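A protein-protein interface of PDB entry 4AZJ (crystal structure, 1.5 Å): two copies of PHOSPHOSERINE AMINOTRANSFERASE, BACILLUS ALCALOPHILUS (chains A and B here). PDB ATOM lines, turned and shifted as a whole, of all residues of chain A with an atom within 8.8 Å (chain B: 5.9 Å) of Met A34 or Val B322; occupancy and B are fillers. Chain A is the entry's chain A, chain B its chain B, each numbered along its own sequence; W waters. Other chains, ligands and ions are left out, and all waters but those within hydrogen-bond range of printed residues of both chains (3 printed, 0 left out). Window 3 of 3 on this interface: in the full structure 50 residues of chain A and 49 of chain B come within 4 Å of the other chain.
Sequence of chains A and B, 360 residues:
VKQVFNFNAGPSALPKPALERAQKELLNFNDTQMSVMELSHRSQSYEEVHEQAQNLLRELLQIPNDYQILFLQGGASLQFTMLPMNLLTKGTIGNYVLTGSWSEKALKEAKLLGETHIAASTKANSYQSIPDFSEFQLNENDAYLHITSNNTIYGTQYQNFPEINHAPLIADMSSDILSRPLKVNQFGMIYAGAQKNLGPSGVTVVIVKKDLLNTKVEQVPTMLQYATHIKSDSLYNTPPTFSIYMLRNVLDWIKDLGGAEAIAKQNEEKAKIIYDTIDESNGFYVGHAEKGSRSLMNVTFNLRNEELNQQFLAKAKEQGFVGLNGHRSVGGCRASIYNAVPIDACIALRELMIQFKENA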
ATOM      1  N   GLU A  25      -7.923  10.505 -24.295  1.00  0.00           N
ATOM      2  CA  GLU A  25      -8.102  11.438 -23.177  1.00  0.00           C
ATOM      3  C   GLU A  25      -8.570  10.723 -21.906  1.00  0.00           C
ATOM      4  O   GLU A  25      -9.046  11.361 -20.978  1.00  0.00           O
ATOM      5  CB  GLU A  25      -9.011  12.612 -23.553  1.00  0.00           C
ATOM      6  CG  GLU A  25     -10.451  12.249 -23.775  1.00  0.00           C
ATOM      7  CD  GLU A  25     -11.272  13.360 -24.455  1.00  0.00           C
ATOM      8  OE1 GLU A  25     -10.697  14.403 -24.798  1.00  0.00           O
ATOM      9  OE2 GLU A  25     -12.490  13.183 -24.690  1.00  0.00           O
ATOM     10  N   LEU A  26      -8.421   9.409 -21.863  1.00  0.00           N
ATOM     11  CA  LEU A  26      -8.936   8.643 -20.721  1.00  0.00           C
ATOM     12  C   LEU A  26      -8.328   9.071 -19.379  1.00  0.00           C
ATOM     13  O   LEU A  26      -8.998   8.948 -18.346  1.00  0.00           O
ATOM     14  CB  LEU A  26      -8.719   7.155 -20.923  1.00  0.00           C
ATOM     15  CG  LEU A  26      -9.686   6.284 -20.104  1.00  0.00           C
ATOM     16  CD1 LEU A  26     -11.093   6.349 -20.707  1.00  0.00           C
ATOM     17  CD2 LEU A  26      -9.162   4.837 -20.019  1.00  0.00           C
ATOM     18  N   LEU A  27      -7.093   9.549 -19.376  1.00  0.00           N
ATOM     19  CA  LEU A  27      -6.443   9.915 -18.119  1.00  0.00           C
ATOM     20  C   LEU A  27      -6.542  11.394 -17.837  1.00  0.00           C
ATOM     21  O   LEU A  27      -6.331  11.822 -16.699  1.00  0.00           O
ATOM     22  CB  LEU A  27      -4.967   9.541 -18.155  1.00  0.00           C
ATOM     23  CG  LEU A  27      -4.607   8.149 -18.654  1.00  0.00           C
ATOM     24  CD1 LEU A  27      -3.091   7.943 -18.575  1.00  0.00           C
ATOM     25  CD2 LEU A  27      -5.334   7.089 -17.868  1.00  0.00           C
ATOM     26  N   ASN A  28      -6.801  12.189 -18.867  1.00  0.00           N
ATOM     27  CA  ASN A  28      -6.801  13.628 -18.766  1.00  0.00           C
ATOM     28  C   ASN A  28      -7.830  14.225 -19.701  1.00  0.00           C
ATOM     29  O   ASN A  28      -7.555  14.529 -20.869  1.00  0.00           O
ATOM     30  CB  ASN A  28      -5.403  14.189 -19.041  1.00  0.00           C
ATOM     31  CG  ASN A  28      -5.371  15.705 -19.020  1.00  0.00           C
ATOM     32  OD1 ASN A  28      -6.282  16.375 -18.526  1.00  0.00           O
ATOM     33  ND2 ASN A  28      -4.284  16.267 -19.548  1.00  0.00           N
ATOM     34  N   PHE A  29      -9.027  14.401 -19.168  1.00  0.00           N
ATOM     35  CA  PHE A  29     -10.128  14.920 -19.958  1.00  0.00           C
ATOM     36  C   PHE A  29     -10.142  16.438 -19.886  1.00  0.00           C
ATOM     37  O   PHE A  29     -10.172  17.003 -18.801  1.00  0.00           O
ATOM     38  CB  PHE A  29     -11.458  14.371 -19.408  1.00  0.00           C
ATOM     39  CG  PHE A  29     -12.661  15.039 -19.987  1.00  0.00           C
ATOM     40  CD1 PHE A  29     -13.043  14.803 -21.301  1.00  0.00           C
ATOM     41  CD2 PHE A  29     -13.367  15.957 -19.252  1.00  0.00           C
ATOM     42  CE1 PHE A  29     -14.155  15.440 -21.832  1.00  0.00           C
ATOM     43  CE2 PHE A  29     -14.475  16.607 -19.789  1.00  0.00           C
ATOM     44  CZ  PHE A  29     -14.847  16.350 -21.074  1.00  0.00           C
ATOM     45  N   ASN A  30     -10.110  17.086 -21.052  1.00  0.00           N
ATOM     46  CA  ASN A  30     -10.342  18.517 -21.161  1.00  0.00           C
ATOM     47  C   ASN A  30      -9.432  19.344 -20.254  1.00  0.00           C
ATOM     48  O   ASN A  30      -9.862  20.322 -19.648  1.00  0.00           O
ATOM     49  CB  ASN A  30     -11.811  18.833 -20.889  1.00  0.00           C
ATOM     50  CG  ASN A  30     -12.221  20.185 -21.429  1.00  0.00           C
ATOM     51  OD1 ASN A  30     -11.575  20.730 -22.320  1.00  0.00           O
ATOM     52  ND2 ASN A  30     -13.293  20.726 -20.892  1.00  0.00           N
ATOM     53  N   ASP A  31      -8.182  18.913 -20.168  1.00  0.00           N
ATOM     54  CA  ASP A  31      -7.144  19.583 -19.384  1.00  0.00           C
ATOM     55  C   ASP A  31      -7.427  19.642 -17.877  1.00  0.00           C
ATOM     56  O   ASP A  31      -6.823  20.425 -17.163  1.00  0.00           O
ATOM     57  CB  ASP A  31      -6.908  20.999 -19.926  1.00  0.00           C
ATOM     58  CG  ASP A  31      -6.428  20.995 -21.368  1.00  0.00           C
ATOM     59  OD1 ASP A  31      -5.465  20.265 -21.676  1.00  0.00           O
ATOM     60  OD2 ASP A  31      -7.031  21.721 -22.185  1.00  0.00           O
ATOM     61  N   THR A  32      -8.328  18.801 -17.384  1.00  0.00           N
ATOM     62  CA  THR A  32      -8.603  18.761 -15.954  1.00  0.00           C
ATOM     63  C   THR A  32      -7.603  17.935 -15.157  1.00  0.00           C
ATOM     64  O   THR A  32      -7.594  17.996 -13.931  1.00  0.00           O
ATOM     65  CB  THR A  32      -9.977  18.148 -15.666  1.00  0.00           C
ATOM     66  OG1 THR A  32      -9.988  16.765 -16.049  1.00  0.00           O
ATOM     67  CG2 THR A  32     -11.101  18.886 -16.381  1.00  0.00           C
ATOM     68  N   GLN A  33      -6.773  17.154 -15.846  1.00  0.00           N
ATOM     69  CA  GLN A  33      -5.869  16.179 -15.253  1.00  0.00           C
ATOM     70  C   GLN A  33      -6.584  15.056 -14.508  1.00  0.00           C
ATOM     71  O   GLN A  33      -5.985  14.375 -13.676  1.00  0.00           O
ATOM     72  CB  GLN A  33      -4.842  16.865 -14.334  1.00  0.00           C
ATOM     73  CG  GLN A  33      -4.264  18.099 -14.956  1.00  0.00           C
ATOM     74  CD  GLN A  33      -3.567  17.827 -16.262  1.00  0.00           C
ATOM     75  OE1 GLN A  33      -2.958  16.770 -16.449  1.00  0.00           O
ATOM     76  NE2 GLN A  33      -3.644  18.792 -17.186  1.00  0.00           N
ATOM     77  N   MET A  34      -7.859  14.858 -14.851  1.00  0.00           N
ATOM     78  CA  MET A  34      -8.645  13.746 -14.335  1.00  0.00           C
ATOM     79  C   MET A  34      -9.297  13.050 -15.515  1.00  0.00           C
ATOM     80  O   MET A  34      -9.618  13.690 -16.515  1.00  0.00           O
ATOM     81  CB  MET A  34      -9.766  14.270 -13.419  1.00  0.00           C
ATOM     82  CG  MET A  34      -9.264  14.872 -12.114  1.00  0.00           C
ATOM     83  SD  MET A  34     -10.583  15.622 -11.122  1.00  0.00           S
ATOM     84  CE  MET A  34     -10.737  17.195 -11.973  1.00  0.00           C
ATOM     85  N   SER A  35      -9.550  11.764 -15.379  1.00  0.00           N
ATOM     86  CA  SER A  35     -10.439  11.078 -16.309  1.00  0.00           C
ATOM     87  C   SER A  35     -11.859  11.622 -16.209  1.00  0.00           C
ATOM     88  O   SER A  35     -12.285  12.076 -15.150  1.00  0.00           O
ATOM     89  CB  SER A  35     -10.473   9.591 -15.971  1.00  0.00           C
ATOM     90  OG  SER A  35     -11.306   8.840 -16.857  1.00  0.00           O
ATOM     91  N   VAL A  36     -12.633  11.512 -17.277  1.00  0.00           N
ATOM     92  CA  VAL A  36     -14.050  11.786 -17.177  1.00  0.00           C
ATOM     93  C   VAL A  36     -14.661  10.951 -16.087  1.00  0.00           C
ATOM     94  O   VAL A  36     -15.604  11.408 -15.408  1.00  0.00           O
ATOM     95  CB  VAL A  36     -14.806  11.398 -18.473  1.00  0.00           C
ATOM     96  CG1 VAL A  36     -16.300  11.130 -18.177  1.00  0.00           C
ATOM     97  CG2 VAL A  36     -14.650  12.457 -19.484  1.00  0.00           C
ATOM     98  N   MET A  37     -14.106   9.750 -15.867  1.00  0.00           N
ATOM     99  CA  MET A  37     -14.590   8.797 -14.838  1.00  0.00           C
ATOM    100  C   MET A  37     -14.347   9.252 -13.397  1.00  0.00           C
ATOM    101  O   MET A  37     -14.815   8.607 -12.439  1.00  0.00           O
ATOM    102  CB  MET A  37     -13.869   7.430 -14.962  1.00  0.00           C
ATOM    103  CG  MET A  37     -14.484   6.630 -16.040  1.00  0.00           C
ATOM    104  SD  MET A  37     -13.688   5.025 -16.101  1.00  0.00           S
ATOM    105  CE  MET A  37     -12.719   5.270 -17.543  1.00  0.00           C
ATOM    106  N   GLU A  38     -13.512  10.269 -13.244  1.00  0.00           N
ATOM    107  CA  GLU A  38     -13.045  10.752 -11.948  1.00  0.00           C
ATOM    108  C   GLU A  38     -13.679  12.085 -11.566  1.00  0.00           C
ATOM    109  O   GLU A  38     -13.393  12.602 -10.482  1.00  0.00           O
ATOM    110  CB  GLU A  38     -11.519  10.891 -11.928  1.00  0.00           C
ATOM    111  CG  GLU A  38     -10.779   9.538 -12.018  1.00  0.00           C
ATOM    112  CD  GLU A  38      -9.283   9.731 -12.114  1.00  0.00           C
ATOM    113  OE1 GLU A  38      -8.823  10.367 -13.072  1.00  0.00           O
ATOM    114  OE2 GLU A  38      -8.545   9.331 -11.209  1.00  0.00           O
ATOM    115  N   LEU A  39     -14.483  12.643 -12.469  1.00  0.00           N
ATOM    116  CA  LEU A  39     -15.178  13.905 -12.221  1.00  0.00           C
ATOM    117  C   LEU A  39     -16.435  13.724 -11.380  1.00  0.00           C
ATOM    118  O   LEU A  39     -17.143  12.741 -11.521  1.00  0.00           O
ATOM    119  CB  LEU A  39     -15.646  14.541 -13.533  1.00  0.00           C
ATOM    120  CG  LEU A  39     -14.574  14.798 -14.594  1.00  0.00           C
ATOM    121  CD1 LEU A  39     -15.255  15.264 -15.886  1.00  0.00           C
ATOM    122  CD2 LEU A  39     -13.549  15.782 -14.103  1.00  0.00           C
ATOM    123  N   SER A  40     -16.730  14.708 -10.547  1.00  0.00           N
ATOM    124  CA  SER A  40     -18.016  14.752  -9.870  1.00  0.00           C
ATOM    125  C   SER A  40     -19.112  15.079 -10.865  1.00  0.00           C
ATOM    126  O   SER A  40     -18.939  15.914 -11.755  1.00  0.00           O
ATOM    127  CB  SER A  40     -18.001  15.824  -8.798  1.00  0.00           C
ATOM    128  OG  SER A  40     -19.303  15.931  -8.220  1.00  0.00           O
ATOM    129  N   SER A  43     -19.943  18.729 -10.874  1.00  0.00           N
ATOM    130  CA  SER A  43     -18.958  19.655 -11.407  1.00  0.00           C
ATOM    131  C   SER A  43     -19.397  20.242 -12.735  1.00  0.00           C
ATOM    132  O   SER A  43     -20.083  19.599 -13.524  1.00  0.00           O
ATOM    133  CB  SER A  43     -17.599  18.964 -11.602  1.00  0.00           C
ATOM    134  OG  SER A  43     -17.609  18.051 -12.711  1.00  0.00           O
ATOM    135  N   GLN A  44     -18.947  21.458 -12.997  1.00  0.00           N
ATOM    136  CA  GLN A  44     -19.124  22.065 -14.309  1.00  0.00           C
ATOM    137  C   GLN A  44     -18.549  21.200 -15.431  1.00  0.00           C
ATOM    138  O   GLN A  44     -19.151  21.083 -16.501  1.00  0.00           O
ATOM    139  CB  GLN A  44     -18.455  23.436 -14.314  1.00  0.00           C
ATOM    140  CG  GLN A  44     -18.474  24.108 -15.677  1.00  0.00           C
ATOM    141  CD  GLN A  44     -18.078  25.573 -15.609  1.00  0.00           C
ATOM    142  OE1 GLN A  44     -18.471  26.291 -14.684  1.00  0.00           O
ATOM    143  NE2 GLN A  44     -17.297  26.023 -16.591  1.00  0.00           N
ATOM    144  N   SER A  45     -17.392  20.583 -15.190  1.00  0.00           N
ATOM    145  CA  SER A  45     -16.731  19.798 -16.225  1.00  0.00           C
ATOM    146  C   SER A  45     -17.627  18.662 -16.688  1.00  0.00           C
ATOM    147  O   SER A  45     -17.733  18.407 -17.881  1.00  0.00           O
ATOM    148  CB  SER A  45     -15.407  19.224 -15.729  1.00  0.00           C
ATOM    149  OG  SER A  45     -14.472  20.264 -15.528  1.00  0.00           O
ATOM    150  N   TYR A  46     -18.262  17.979 -15.742  1.00  0.00           N
ATOM    151  CA  TYR A  46     -19.202  16.932 -16.112  1.00  0.00           C
ATOM    152  C   TYR A  46     -20.503  17.498 -16.702  1.00  0.00           C
ATOM    153  O   TYR A  46     -21.021  16.998 -17.722  1.00  0.00           O
ATOM    154  CB  TYR A  46     -19.509  15.921 -14.958  1.00  0.00           C
ATOM    155  CG  TYR A  46     -20.549  14.987 -15.472  1.00  0.00           C
ATOM    156  CD1 TYR A  46     -20.207  14.011 -16.407  1.00  0.00           C
ATOM    157  CD2 TYR A  46     -21.886  15.151 -15.128  1.00  0.00           C
ATOM    158  CE1 TYR A  46     -21.181  13.240 -17.008  1.00  0.00           C
ATOM    159  CE2 TYR A  46     -22.875  14.377 -15.718  1.00  0.00           C
ATOM    160  CZ  TYR A  46     -22.503  13.423 -16.650  1.00  0.00           C
ATOM    161  OH  TYR A  46     -23.483  12.665 -17.240  1.00  0.00           O
ATOM    162  N   VAL B   4      -3.053  19.022  -9.653  1.00  0.00           N
ATOM    163  CA  VAL B   4      -4.467  18.783  -9.334  1.00  0.00           C
ATOM    164  C   VAL B   4      -4.556  17.745  -8.246  1.00  0.00           C
ATOM    165  O   VAL B   4      -3.900  16.707  -8.302  1.00  0.00           O
ATOM    166  CB  VAL B   4      -5.248  18.342 -10.582  1.00  0.00           C
ATOM    167  CG1 VAL B   4      -6.658  17.879 -10.227  1.00  0.00           C
ATOM    168  CG2 VAL B   4      -5.274  19.525 -11.583  1.00  0.00           C
ATOM    169  N   PHE B   5      -5.346  18.049  -7.219  1.00  0.00           N
ATOM    170  CA  PHE B   5      -5.563  17.097  -6.139  1.00  0.00           C
ATOM    171  C   PHE B   5      -7.043  16.764  -6.092  1.00  0.00           C
ATOM    172  O   PHE B   5      -7.877  17.644  -5.827  1.00  0.00           O
ATOM    173  CB  PHE B   5      -5.107  17.678  -4.806  1.00  0.00           C
ATOM    174  CG  PHE B   5      -3.680  18.124  -4.812  1.00  0.00           C
ATOM    175  CD1 PHE B   5      -2.666  17.197  -4.799  1.00  0.00           C
ATOM    176  CD2 PHE B   5      -3.375  19.468  -4.911  1.00  0.00           C
ATOM    177  CE1 PHE B   5      -1.327  17.611  -4.822  1.00  0.00           C
ATOM    178  CE2 PHE B   5      -2.047  19.882  -4.939  1.00  0.00           C
ATOM    179  CZ  PHE B   5      -1.049  18.951  -4.916  1.00  0.00           C
ATOM    180  N   ASN B   6      -7.362  15.492  -6.317  1.00  0.00           N
ATOM    181  CA  ASN B   6      -8.742  15.081  -6.510  1.00  0.00           C
ATOM    182  C   ASN B   6      -9.366  14.502  -5.252  1.00  0.00           C
ATOM    183  O   ASN B   6      -9.196  13.312  -4.908  1.00  0.00           O
ATOM    184  CB  ASN B   6      -8.843  14.095  -7.684  1.00  0.00           C
ATOM    185  CG  ASN B   6     -10.266  13.728  -7.999  1.00  0.00           C
ATOM    186  OD1 ASN B   6     -11.188  14.239  -7.368  1.00  0.00           O
ATOM    187  ND2 ASN B   6     -10.462  12.848  -8.956  1.00  0.00           N
ATOM    188  N   PHE B   7     -10.133  15.361  -4.576  1.00  0.00           N
ATOM    189  CA  PHE B   7     -10.902  15.014  -3.385  1.00  0.00           C
ATOM    190  C   PHE B   7     -12.379  14.881  -3.653  1.00  0.00           C
ATOM    191  O   PHE B   7     -13.184  15.006  -2.741  1.00  0.00           O
ATOM    192  CB  PHE B   7     -10.647  16.052  -2.285  1.00  0.00           C
ATOM    193  CG  PHE B   7      -9.250  15.976  -1.692  1.00  0.00           C
ATOM    194  CD1 PHE B   7      -8.985  15.091  -0.672  1.00  0.00           C
ATOM    195  CD2 PHE B   7      -8.221  16.799  -2.147  1.00  0.00           C
ATOM    196  CE1 PHE B   7      -7.710  14.989  -0.101  1.00  0.00           C
ATOM    197  CE2 PHE B   7      -6.935  16.712  -1.581  1.00  0.00           C
ATOM    198  CZ  PHE B   7      -6.690  15.796  -0.567  1.00  0.00           C
ATOM    199  N   ASN B   8     -12.735  14.586  -4.894  1.00  0.00           N
ATOM    200  CA  ASN B   8     -14.137  14.367  -5.237  1.00  0.00           C
ATOM    201  C   ASN B   8     -14.770  13.261  -4.410  1.00  0.00           C
ATOM    202  O   ASN B   8     -14.157  12.223  -4.106  1.00  0.00           O
ATOM    203  CB  ASN B   8     -14.299  14.070  -6.714  1.00  0.00           C
ATOM    204  CG  ASN B   8     -14.260  15.303  -7.584  1.00  0.00           C
ATOM    205  OD1 ASN B   8     -14.562  16.395  -7.133  1.00  0.00           O
ATOM    206  ND2 ASN B   8     -13.889  15.132  -8.845  1.00  0.00           N
ATOM    207  N   ALA B 316      -8.216  26.979  -1.974  1.00  0.00           N
ATOM    208  CA  ALA B 316      -8.064  25.590  -2.366  1.00  0.00           C
ATOM    209  C   ALA B 316      -8.255  25.416  -3.863  1.00  0.00           C
ATOM    210  O   ALA B 316      -7.457  24.736  -4.532  1.00  0.00           O
ATOM    211  CB  ALA B 316      -9.042  24.706  -1.573  1.00  0.00           C
ATOM    212  N   GLY B 320      -5.496  24.172  -7.006  1.00  0.00           N
ATOM    213  CA  GLY B 320      -5.655  22.921  -7.724  1.00  0.00           C
ATOM    214  C   GLY B 320      -6.411  21.820  -7.011  1.00  0.00           C
ATOM    215  O   GLY B 320      -6.447  20.683  -7.515  1.00  0.00           O
ATOM    216  N   PHE B 321      -7.001  22.132  -5.871  1.00  0.00           N
ATOM    217  CA  PHE B 321      -7.767  21.155  -5.135  1.00  0.00           C
ATOM    218  C   PHE B 321      -9.162  21.086  -5.735  1.00  0.00           C
ATOM    219  O   PHE B 321      -9.816  22.106  -5.936  1.00  0.00           O
ATOM    220  CB  PHE B 321      -7.839  21.498  -3.629  1.00  0.00           C
ATOM    221  CG  PHE B 321      -6.517  21.368  -2.945  1.00  0.00           C
ATOM    222  CD1 PHE B 321      -5.562  22.361  -3.068  1.00  0.00           C
ATOM    223  CD2 PHE B 321      -6.217  20.231  -2.207  1.00  0.00           C
ATOM    224  CE1 PHE B 321      -4.326  22.222  -2.461  1.00  0.00           C
ATOM    225  CE2 PHE B 321      -4.955  20.067  -1.610  1.00  0.00           C
ATOM    226  CZ  PHE B 321      -4.010  21.057  -1.739  1.00  0.00           C
ATOM    227  N   VAL B 322      -9.619  19.864  -5.988  1.00  0.00           N
ATOM    228  CA  VAL B 322     -10.926  19.620  -6.587  1.00  0.00           C
ATOM    229  C   VAL B 322     -11.821  18.874  -5.611  1.00  0.00           C
ATOM    230  O   VAL B 322     -11.399  17.892  -5.001  1.00  0.00           O
ATOM    231  CB  VAL B 322     -10.744  18.761  -7.856  1.00  0.00           C
ATOM    232  CG1 VAL B 322     -12.081  18.375  -8.478  1.00  0.00           C
ATOM    233  CG2 VAL B 322      -9.901  19.558  -8.867  1.00  0.00           C
ATOM    234  N   GLY B 323     -13.059  19.339  -5.469  1.00  0.00           N
ATOM    235  CA  GLY B 323     -14.054  18.626  -4.698  1.00  0.00           C
ATOM    236  C   GLY B 323     -14.110  18.860  -3.196  1.00  0.00           C
ATOM    237  O   GLY B 323     -14.804  18.143  -2.494  1.00  0.00           O
ATOM    238  N   LEU B 324     -13.364  19.841  -2.678  1.00  0.00           N
ATOM    239  CA  LEU B 324     -13.325  20.073  -1.234  1.00  0.00           C
ATOM    240  C   LEU B 324     -14.550  20.757  -0.660  1.00  0.00           C
ATOM    241  O   LEU B 324     -14.783  20.686   0.549  1.00  0.00           O
ATOM    242  CB  LEU B 324     -12.103  20.881  -0.797  1.00  0.00           C
ATOM    243  CG  LEU B 324     -10.763  20.187  -0.863  1.00  0.00           C
ATOM    244  CD1 LEU B 324      -9.690  21.144  -0.408  1.00  0.00           C
ATOM    245  CD2 LEU B 324     -10.772  18.916  -0.023  1.00  0.00           C
HETATM  246  O   HOH W   1     -14.903  17.229 -10.743  1.00  0.00           O
HETATM  247  O   HOH W   2     -17.327  15.617  -5.419  1.00  0.00           O
HETATM  248  O   HOH W   3      -7.822  11.718  -9.955  1.00  0.00           O
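Of the 11 printed residues of chain B, 4 touch a printed residue of chain A. Hydrophobic or aromatic side chains of chain B within 4 Å of the printed part of chain A: Val B4 and Val B322. Of the 20 printed residues of chain A, 6 touch a printed residue of chain B. Hydrophobic or aromatic side chains of chain A within 4 Å of the printed part of chain B: Met A34. Along chain A the printed residues that touch a printed residue of chain B span positions 32 to 40.
OD1 of Asn A28 lies within hydrogen-bond range of N of Thr A32. N of Gln A33 sits at hydrogen-bond distance from OD1 of Asn A28 (2.8 Å). The backbone NH (N) of Phe A29 sits at hydrogen-bond distance from the backbone carbonyl oxygen (O) of Met A34, 2.8 Å away. The side-chain carboxylate (OE1) of Glu A38 sits at hydrogen-bond distance from the backbone NH (N) of Ser A35 (2.8 Å). The backbone carbonyl oxygen of Ser A40 sits at hydrogen-bond distance from the side-chain hydroxyl of Ser A43 (2.7 Å). The backbone NH (N) of Asn B8 is in hydrogen-bond range of the side-chain amide oxygen (OD1) of Asn B6, 2.9 Å away.
Printed residues of chain B within 4 Å of Thr A32: Val B4 (3.6 Å). Met A34 touches just these residues of chain B: Asn B6 and Val B322. Of the printed residues of chain B, Glu A38 touches Asn B6 and Asn B8. Of the printed residues of chain B, Leu A39 touches Asn B8 (3.8 Å). Of the printed residues of chain A, Val B4 touches Thr A32 and Gln A33. Of the printed residues of chain A, Asn B8 touches Glu A38, Leu A39 and Ser A40. Gly B323 touches none of the printed residues of chain A. The nearest residue of chain B that does not touch Met A34 is Asn B8 (4.04 Å).
SD of Met A34 sits at hydrogen-bond distance from ND2 of Asn B6 (3.5 Å). The backbone carbonyl oxygen of Glu A38 is in hydrogen-bond range of the side-chain amide nitrogen of Asn B6 (3.3 Å). The backbone carbonyl oxygen (O) of Glu A38 lies within hydrogen-bond range of the side-chain amide nitrogen (ND2) of Asn B8 (3.1 Å). ND2 of Asn B8 sits close to N of Ser A40.
Among the printed residues, pairs that only touch across the chains: Thr A32 with Val B4 (3.6 Å), Gln A33 with Val B4 (3.8 Å), Leu A39 with Asn B8 (3.8 Å) and Met A34 with Val B322 (3.9 Å).
No position is printed for both chains. Of the 8 pairs that touch across the chains among the printed residues, none has its exchanged pair printed and touching as well.
Water W3 lies within hydrogen-bond range of the side-chain carboxylate (OE2) of Glu A38 (2.8 Å) and the side-chain amide nitrogen (ND2) of Asn B6 (3.0 Å). Water W1 lies within hydrogen-bond range of the side-chain amide nitrogen (ND2) of Asn B8 (3.0 Å), the backbone NH (N) of Ser A40 (3.1 Å) and the side-chain hydroxyl (OG) of Ser A43 (3.4 Å). Water W2 lies within hydrogen-bond range of OD1 of Asn B8 and OG of Ser A40.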
